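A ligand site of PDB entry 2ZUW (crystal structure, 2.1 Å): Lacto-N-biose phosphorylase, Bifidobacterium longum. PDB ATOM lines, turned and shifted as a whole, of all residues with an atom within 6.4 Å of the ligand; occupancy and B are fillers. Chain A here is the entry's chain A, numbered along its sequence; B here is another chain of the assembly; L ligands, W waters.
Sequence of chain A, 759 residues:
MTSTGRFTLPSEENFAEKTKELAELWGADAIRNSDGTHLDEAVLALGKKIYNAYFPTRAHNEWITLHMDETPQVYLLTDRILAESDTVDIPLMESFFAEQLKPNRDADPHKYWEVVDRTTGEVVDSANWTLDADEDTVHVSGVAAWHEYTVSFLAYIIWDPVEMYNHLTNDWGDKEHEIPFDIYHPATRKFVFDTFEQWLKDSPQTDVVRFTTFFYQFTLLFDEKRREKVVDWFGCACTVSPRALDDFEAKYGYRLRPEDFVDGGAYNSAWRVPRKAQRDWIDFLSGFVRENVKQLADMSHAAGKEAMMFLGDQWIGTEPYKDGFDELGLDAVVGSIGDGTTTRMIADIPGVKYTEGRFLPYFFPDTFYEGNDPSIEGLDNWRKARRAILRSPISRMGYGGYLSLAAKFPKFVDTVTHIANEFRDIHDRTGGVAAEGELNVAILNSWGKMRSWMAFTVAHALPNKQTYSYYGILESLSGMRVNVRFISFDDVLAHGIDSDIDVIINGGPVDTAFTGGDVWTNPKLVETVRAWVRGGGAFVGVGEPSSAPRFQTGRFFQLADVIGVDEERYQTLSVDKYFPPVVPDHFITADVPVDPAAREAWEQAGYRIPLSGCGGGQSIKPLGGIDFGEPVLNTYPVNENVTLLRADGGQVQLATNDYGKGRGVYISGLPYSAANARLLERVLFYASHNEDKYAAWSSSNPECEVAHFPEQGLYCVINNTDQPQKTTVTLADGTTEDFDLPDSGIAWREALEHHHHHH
N of Asp 313 sits at hydrogen-bond distance from O5 of the ligand, 3.0 Å away.
The side-chain carboxylate of Asp 313 is in hydrogen-bond range of an oxygen (O2) of the ligand.
The indole nitrogen (NE1) of Trp 233 sits at hydrogen-bond distance from an oxygen (O5) of the ligand, 2.9 Å away.
O of Asp 313 is in hydrogen-bond range of N of Phe 218 (3.3 Å).
O of Trp 233 lies within hydrogen-bond range of NE1 of Trp 315, 3.0 Å away.
OG of Ser 612 of chain B lies within hydrogen-bond range of OE1 of Glu 228 (2.5 Å).
Merely in contact with the ligand: Tyr 165 (3.5 Å), Phe 218 (3.4 Å), Phe 310 (3.6 Å), Leu 311 (3.4 Å), Gly 312 (3.0 Å), Ser 336 (3.6 Å), His 460 (3.95 Å) and Ser 612 of chain B (3.9 Å).
The nearest printed residue that does not touch the ligand is Val 162 (4.2 Å).
Water W10 lies within hydrogen-bond range of O6 of the ligand and O of His 460.
Water W8 bridges O3 of the ligand (2.7 Å) and OD1 of Asn 166 (3.0 Å).
Water W2 lies within hydrogen-bond range of O4 of the ligand (2.8 Å) and OE1 of Glu 228 (2.8 Å).
Water W6 lies within hydrogen-bond range of OG of Ser 336 (2.7 Å) and N1 of the ligand (3.0 Å).
Water W7 bridges O4 of the ligand and OH of Tyr 165.
Water W5 bridges the side-chain carboxylate of Asp 313 (2.8 Å) and an oxygen (O2) of the ligand (3.4 Å).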
ATOM      1  N   VAL A 162      20.055 -24.590 -12.162  1.00  0.00           N
ATOM      2  CA  VAL A 162      19.963 -23.216 -11.638  1.00  0.00           C
ATOM      3  C   VAL A 162      18.659 -22.502 -12.081  1.00  0.00           C
ATOM      4  O   VAL A 162      18.005 -21.822 -11.273  1.00  0.00           O
ATOM      5  CB  VAL A 162      21.217 -22.392 -11.953  1.00  0.00           C
ATOM      6  CG1 VAL A 162      21.009 -20.967 -11.506  1.00  0.00           C
ATOM      7  CG2 VAL A 162      22.427 -22.974 -11.221  1.00  0.00           C
ATOM      8  N   TYR A 165      16.083 -23.944  -9.846  1.00  0.00           N
ATOM      9  CA  TYR A 165      16.214 -23.288  -8.548  1.00  0.00           C
ATOM     10  C   TYR A 165      15.438 -21.956  -8.576  1.00  0.00           C
ATOM     11  O   TYR A 165      14.579 -21.723  -7.718  1.00  0.00           O
ATOM     12  CB  TYR A 165      17.675 -23.032  -8.136  1.00  0.00           C
ATOM     13  CG  TYR A 165      17.767 -22.141  -6.891  1.00  0.00           C
ATOM     14  CD1 TYR A 165      17.563 -22.663  -5.603  1.00  0.00           C
ATOM     15  CD2 TYR A 165      18.032 -20.779  -7.019  1.00  0.00           C
ATOM     16  CE1 TYR A 165      17.619 -21.829  -4.460  1.00  0.00           C
ATOM     17  CE2 TYR A 165      18.102 -19.942  -5.887  1.00  0.00           C
ATOM     18  CZ  TYR A 165      17.890 -20.483  -4.622  1.00  0.00           C
ATOM     19  OH  TYR A 165      17.952 -19.654  -3.529  1.00  0.00           O
ATOM     20  N   ASN A 166      15.740 -21.097  -9.537  1.00  0.00           N
ATOM     21  CA  ASN A 166      15.086 -19.804  -9.623  1.00  0.00           C
ATOM     22  C   ASN A 166      13.568 -19.880  -9.860  1.00  0.00           C
ATOM     23  O   ASN A 166      12.822 -19.106  -9.269  1.00  0.00           O
ATOM     24  CB  ASN A 166      15.769 -18.935 -10.659  1.00  0.00           C
ATOM     25  CG  ASN A 166      17.156 -18.515 -10.233  1.00  0.00           C
ATOM     26  OD1 ASN A 166      18.120 -18.811 -10.904  1.00  0.00           O
ATOM     27  ND2 ASN A 166      17.265 -17.880  -9.076  1.00  0.00           N
ATOM     28  N   PHE A 218      27.563 -27.421 -11.541  1.00  0.00           N
ATOM     29  CA  PHE A 218      27.887 -28.056 -10.254  1.00  0.00           C
ATOM     30  C   PHE A 218      26.761 -28.940  -9.752  1.00  0.00           C
ATOM     31  O   PHE A 218      25.596 -28.627  -9.936  1.00  0.00           O
ATOM     32  CB  PHE A 218      28.370 -27.042  -9.192  1.00  0.00           C
ATOM     33  CG  PHE A 218      27.300 -26.094  -8.652  1.00  0.00           C
ATOM     34  CD1 PHE A 218      26.377 -26.526  -7.667  1.00  0.00           C
ATOM     35  CD2 PHE A 218      27.268 -24.768  -9.058  1.00  0.00           C
ATOM     36  CE1 PHE A 218      25.422 -25.642  -7.155  1.00  0.00           C
ATOM     37  CE2 PHE A 218      26.320 -23.875  -8.552  1.00  0.00           C
ATOM     38  CZ  PHE A 218      25.400 -24.297  -7.597  1.00  0.00           C
ATOM     39  N   LEU A 220      23.762 -30.434  -8.453  1.00  0.00           N
ATOM     40  CA  LEU A 220      22.568 -29.833  -7.856  1.00  0.00           C
ATOM     41  C   LEU A 220      21.325 -30.605  -8.276  1.00  0.00           C
ATOM     42  O   LEU A 220      20.766 -30.376  -9.356  1.00  0.00           O
ATOM     43  CB  LEU A 220      22.481 -28.349  -8.219  1.00  0.00           C
ATOM     44  CG  LEU A 220      21.353 -27.478  -7.651  1.00  0.00           C
ATOM     45  CD1 LEU A 220      21.324 -27.457  -6.105  1.00  0.00           C
ATOM     46  CD2 LEU A 220      21.441 -26.088  -8.206  1.00  0.00           C
ATOM     47  N   GLU A 228      16.040 -29.399  -2.446  1.00  0.00           N
ATOM     48  CA  GLU A 228      17.403 -29.844  -2.727  1.00  0.00           C
ATOM     49  C   GLU A 228      17.624 -31.203  -2.064  1.00  0.00           C
ATOM     50  O   GLU A 228      17.273 -31.399  -0.892  1.00  0.00           O
ATOM     51  CB  GLU A 228      18.403 -28.837  -2.211  1.00  0.00           C
ATOM     52  CG  GLU A 228      19.799 -29.005  -2.820  1.00  0.00           C
ATOM     53  CD  GLU A 228      20.782 -28.138  -2.117  1.00  0.00           C
ATOM     54  OE1 GLU A 228      21.079 -27.042  -2.636  1.00  0.00           O
ATOM     55  OE2 GLU A 228      21.210 -28.545  -1.006  1.00  0.00           O
ATOM     56  N   VAL A 231      23.827 -31.448  -3.160  1.00  0.00           N
ATOM     57  CA  VAL A 231      24.524 -30.271  -3.666  1.00  0.00           C
ATOM     58  C   VAL A 231      25.999 -30.346  -3.341  1.00  0.00           C
ATOM     59  O   VAL A 231      26.369 -30.685  -2.205  1.00  0.00           O
ATOM     60  CB  VAL A 231      23.931 -28.926  -3.114  1.00  0.00           C
ATOM     61  CG1 VAL A 231      24.253 -28.725  -1.630  1.00  0.00           C
ATOM     62  CG2 VAL A 231      24.450 -27.728  -3.932  1.00  0.00           C
ATOM     63  N   TRP A 233      29.174 -27.616  -4.473  1.00  0.00           N
ATOM     64  CA  TRP A 233      29.557 -26.483  -5.307  1.00  0.00           C
ATOM     65  C   TRP A 233      30.714 -26.869  -6.239  1.00  0.00           C
ATOM     66  O   TRP A 233      30.911 -26.225  -7.274  1.00  0.00           O
ATOM     67  CB  TRP A 233      29.894 -25.258  -4.467  1.00  0.00           C
ATOM     68  CG  TRP A 233      30.021 -24.032  -5.302  1.00  0.00           C
ATOM     69  CD1 TRP A 233      29.072 -23.501  -6.149  1.00  0.00           C
ATOM     70  CD2 TRP A 233      31.155 -23.157  -5.363  1.00  0.00           C
ATOM     71  NE1 TRP A 233      29.553 -22.365  -6.731  1.00  0.00           N
ATOM     72  CE2 TRP A 233      30.834 -22.140  -6.286  1.00  0.00           C
ATOM     73  CE3 TRP A 233      32.407 -23.147  -4.741  1.00  0.00           C
ATOM     74  CZ2 TRP A 233      31.722 -21.101  -6.588  1.00  0.00           C
ATOM     75  CZ3 TRP A 233      33.315 -22.117  -5.051  1.00  0.00           C
ATOM     76  CH2 TRP A 233      32.954 -21.112  -5.978  1.00  0.00           C
ATOM     77  N   PHE A 310      31.787 -16.104 -14.861  1.00  0.00           N
ATOM     78  CA  PHE A 310      31.190 -16.189 -13.539  1.00  0.00           C
ATOM     79  C   PHE A 310      31.784 -17.388 -12.800  1.00  0.00           C
ATOM     80  O   PHE A 310      31.745 -18.508 -13.297  1.00  0.00           O
ATOM     81  CB  PHE A 310      29.685 -16.348 -13.640  1.00  0.00           C
ATOM     82  CG  PHE A 310      28.980 -16.462 -12.292  1.00  0.00           C
ATOM     83  CD1 PHE A 310      29.208 -15.535 -11.283  1.00  0.00           C
ATOM     84  CD2 PHE A 310      28.068 -17.505 -12.073  1.00  0.00           C
ATOM     85  CE1 PHE A 310      28.540 -15.636 -10.060  1.00  0.00           C
ATOM     86  CE2 PHE A 310      27.383 -17.616 -10.853  1.00  0.00           C
ATOM     87  CZ  PHE A 310      27.633 -16.686  -9.845  1.00  0.00           C
ATOM     88  N   LEU A 311      32.374 -17.140 -11.630  1.00  0.00           N
ATOM     89  CA  LEU A 311      32.855 -18.211 -10.744  1.00  0.00           C
ATOM     90  C   LEU A 311      31.662 -18.856 -10.018  1.00  0.00           C
ATOM     91  O   LEU A 311      31.364 -18.540  -8.867  1.00  0.00           O
ATOM     92  CB  LEU A 311      33.836 -17.614  -9.712  1.00  0.00           C
ATOM     93  CG  LEU A 311      34.608 -18.643  -8.898  1.00  0.00           C
ATOM     94  CD1 LEU A 311      35.601 -19.409  -9.812  1.00  0.00           C
ATOM     95  CD2 LEU A 311      35.306 -18.021  -7.696  1.00  0.00           C
ATOM     96  N   GLY A 312      30.975 -19.751 -10.706  1.00  0.00           N
ATOM     97  CA  GLY A 312      29.747 -20.327 -10.182  1.00  0.00           C
ATOM     98  C   GLY A 312      28.976 -21.030 -11.285  1.00  0.00           C
ATOM     99  O   GLY A 312      29.412 -21.050 -12.444  1.00  0.00           O
ATOM    100  N   ASP A 313      27.824 -21.578 -10.928  1.00  0.00           N
ATOM    101  CA  ASP A 313      26.930 -22.291 -11.861  1.00  0.00           C
ATOM    102  C   ASP A 313      27.679 -23.306 -12.743  1.00  0.00           C
ATOM    103  O   ASP A 313      28.239 -24.254 -12.199  1.00  0.00           O
ATOM    104  CB  ASP A 313      26.058 -21.327 -12.648  1.00  0.00           C
ATOM    105  CG  ASP A 313      25.186 -20.443 -11.731  1.00  0.00           C
ATOM    106  OD1 ASP A 313      25.150 -20.659 -10.494  1.00  0.00           O
ATOM    107  OD2 ASP A 313      24.539 -19.511 -12.264  1.00  0.00           O
ATOM    108  N   TRP A 315      30.559 -23.945 -13.941  1.00  0.00           N
ATOM    109  CA  TRP A 315      31.990 -23.671 -13.903  1.00  0.00           C
ATOM    110  C   TRP A 315      32.863 -24.936 -13.761  1.00  0.00           C
ATOM    111  O   TRP A 315      34.087 -24.848 -13.701  1.00  0.00           O
ATOM    112  CB  TRP A 315      32.308 -22.692 -12.766  1.00  0.00           C
ATOM    113  CG  TRP A 315      32.276 -23.315 -11.368  1.00  0.00           C
ATOM    114  CD1 TRP A 315      31.189 -23.846 -10.712  1.00  0.00           C
ATOM    115  CD2 TRP A 315      33.377 -23.436 -10.472  1.00  0.00           C
ATOM    116  NE1 TRP A 315      31.551 -24.285  -9.460  1.00  0.00           N
ATOM    117  CE2 TRP A 315      32.891 -24.057  -9.290  1.00  0.00           C
ATOM    118  CE3 TRP A 315      34.731 -23.096 -10.552  1.00  0.00           C
ATOM    119  CZ2 TRP A 315      33.720 -24.328  -8.202  1.00  0.00           C
ATOM    120  CZ3 TRP A 315      35.550 -23.354  -9.455  1.00  0.00           C
ATOM    121  CH2 TRP A 315      35.039 -23.962  -8.298  1.00  0.00           C
ATOM    122  N   GLY A 335      32.528 -12.930  -9.503  1.00  0.00           N
ATOM    123  CA  GLY A 335      31.923 -13.889  -8.565  1.00  0.00           C
ATOM    124  C   GLY A 335      31.042 -13.215  -7.517  1.00  0.00           C
ATOM    125  O   GLY A 335      31.059 -12.000  -7.372  1.00  0.00           O
ATOM    126  N   SER A 336      30.262 -14.022  -6.788  1.00  0.00           N
ATOM    127  CA  SER A 336      29.419 -13.495  -5.692  1.00  0.00           C
ATOM    128  C   SER A 336      30.239 -13.272  -4.440  1.00  0.00           C
ATOM    129  O   SER A 336      30.965 -14.162  -3.983  1.00  0.00           O
ATOM    130  CB  SER A 336      28.282 -14.452  -5.305  1.00  0.00           C
ATOM    131  OG  SER A 336      27.892 -15.247  -6.394  1.00  0.00           O
ATOM    132  N   ALA A 459      27.711 -26.048   0.052  1.00  0.00           N
ATOM    133  CA  ALA A 459      27.032 -25.044  -0.788  1.00  0.00           C
ATOM    134  C   ALA A 459      27.775 -23.722  -0.620  1.00  0.00           C
ATOM    135  O   ALA A 459      28.191 -23.386   0.479  1.00  0.00           O
ATOM    136  CB  ALA A 459      25.581 -24.892  -0.385  1.00  0.00           C
ATOM    137  N   HIS A 460      27.932 -22.979  -1.720  1.00  0.00           N
ATOM    138  CA  HIS A 460      28.631 -21.689  -1.721  1.00  0.00           C
ATOM    139  C   HIS A 460      28.091 -20.705  -0.666  1.00  0.00           C
ATOM    140  O   HIS A 460      26.886 -20.429  -0.609  1.00  0.00           O
ATOM    141  CB  HIS A 460      28.569 -21.064  -3.121  1.00  0.00           C
ATOM    142  CG  HIS A 460      29.437 -19.847  -3.288  1.00  0.00           C
ATOM    143  ND1 HIS A 460      28.964 -18.566  -3.093  1.00  0.00           N
ATOM    144  CD2 HIS A 460      30.735 -19.706  -3.662  1.00  0.00           C
ATOM    145  CE1 HIS A 460      29.925 -17.701  -3.332  1.00  0.00           C
ATOM    146  NE2 HIS A 460      31.018 -18.366  -3.676  1.00  0.00           N
ATOM    147  N   LEU A 462      27.376 -20.899   2.377  1.00  0.00           N
ATOM    148  CA  LEU A 462      26.412 -21.398   3.395  1.00  0.00           C
ATOM    149  C   LEU A 462      27.028 -22.377   4.420  1.00  0.00           C
ATOM    150  O   LEU A 462      26.715 -23.584   4.437  1.00  0.00           O
ATOM    151  CB  LEU A 462      25.176 -22.006   2.722  1.00  0.00           C
ATOM    152  CG  LEU A 462      24.294 -21.037   1.916  1.00  0.00           C
ATOM    153  CD1 LEU A 462      23.227 -21.815   1.158  1.00  0.00           C
ATOM    154  CD2 LEU A 462      23.639 -19.978   2.839  1.00  0.00           C
ATOM    155  N   SER B 612      19.879 -24.586   1.009  1.00  0.00           N
ATOM    156  CA  SER B 612      20.873 -25.310   0.225  1.00  0.00           C
ATOM    157  C   SER B 612      22.046 -25.788   1.096  1.00  0.00           C
ATOM    158  O   SER B 612      22.632 -24.981   1.821  1.00  0.00           O
ATOM    159  CB  SER B 612      21.415 -24.441  -0.903  1.00  0.00           C
ATOM    160  OG  SER B 612      22.390 -25.181  -1.624  1.00  0.00           O
HETATM  161  C1  LIG L   1      24.872 -21.078  -5.699  1.00  0.00           C
HETATM  162  C2  LIG L   1      25.042 -20.320  -7.014  1.00  0.00           C
HETATM  163  C3  LIG L   1      23.745 -19.584  -7.397  1.00  0.00           C
HETATM  164  C4  LIG L   1      22.534 -20.513  -7.280  1.00  0.00           C
HETATM  165  C5  LIG L   1      22.516 -21.260  -5.936  1.00  0.00           C
HETATM  166  C6  LIG L   1      21.409 -22.307  -5.866  1.00  0.00           C
HETATM  167  C7  LIG L   1      27.397 -19.690  -7.349  1.00  0.00           C
HETATM  168  C8  LIG L   1      28.463 -18.696  -7.012  1.00  0.00           C
HETATM  169  O1  LIG L   1      23.751 -21.923  -5.750  1.00  0.00           O
HETATM  170  O2  LIG L   1      23.805 -19.140  -8.731  1.00  0.00           O
HETATM  171  O3  LIG L   1      21.366 -19.738  -7.474  1.00  0.00           O
HETATM  172  O4  LIG L   1      21.352 -22.969  -4.608  1.00  0.00           O
HETATM  173  O5  LIG L   1      27.646 -20.679  -8.051  1.00  0.00           O
HETATM  174  N1  LIG L   1      26.191 -19.434  -6.846  1.00  0.00           N
HETATM  175  O6  LIG L   1      24.702 -20.167  -4.628  1.00  0.00           O
HETATM  176  O   HOH W   1      24.606 -18.723  -1.683  1.00  0.00           O
HETATM  177  O   HOH W   2      19.614 -25.043  -4.028  1.00  0.00           O
HETATM  178  O   HOH W   3      23.893 -16.643  -8.793  1.00  0.00           O
HETATM  179  O   HOH W   4      20.908 -18.061  -5.647  1.00  0.00           O
HETATM  180  O   HOH W   5      22.663 -17.607 -11.487  1.00  0.00           O
HETATM  181  O   HOH W   6      25.699 -16.687  -5.618  1.00  0.00           O
HETATM  182  O   HOH W   7      20.354 -21.337  -2.206  1.00  0.00           O
HETATM  183  O   HOH W   8      20.791 -18.136  -9.615  1.00  0.00           O
HETATM  184  O   HOH W   9      23.768 -23.548  -3.148  1.00  0.00           O
HETATM  185  O   HOH W  10      24.866 -21.196  -2.274  1.00  0.00           O
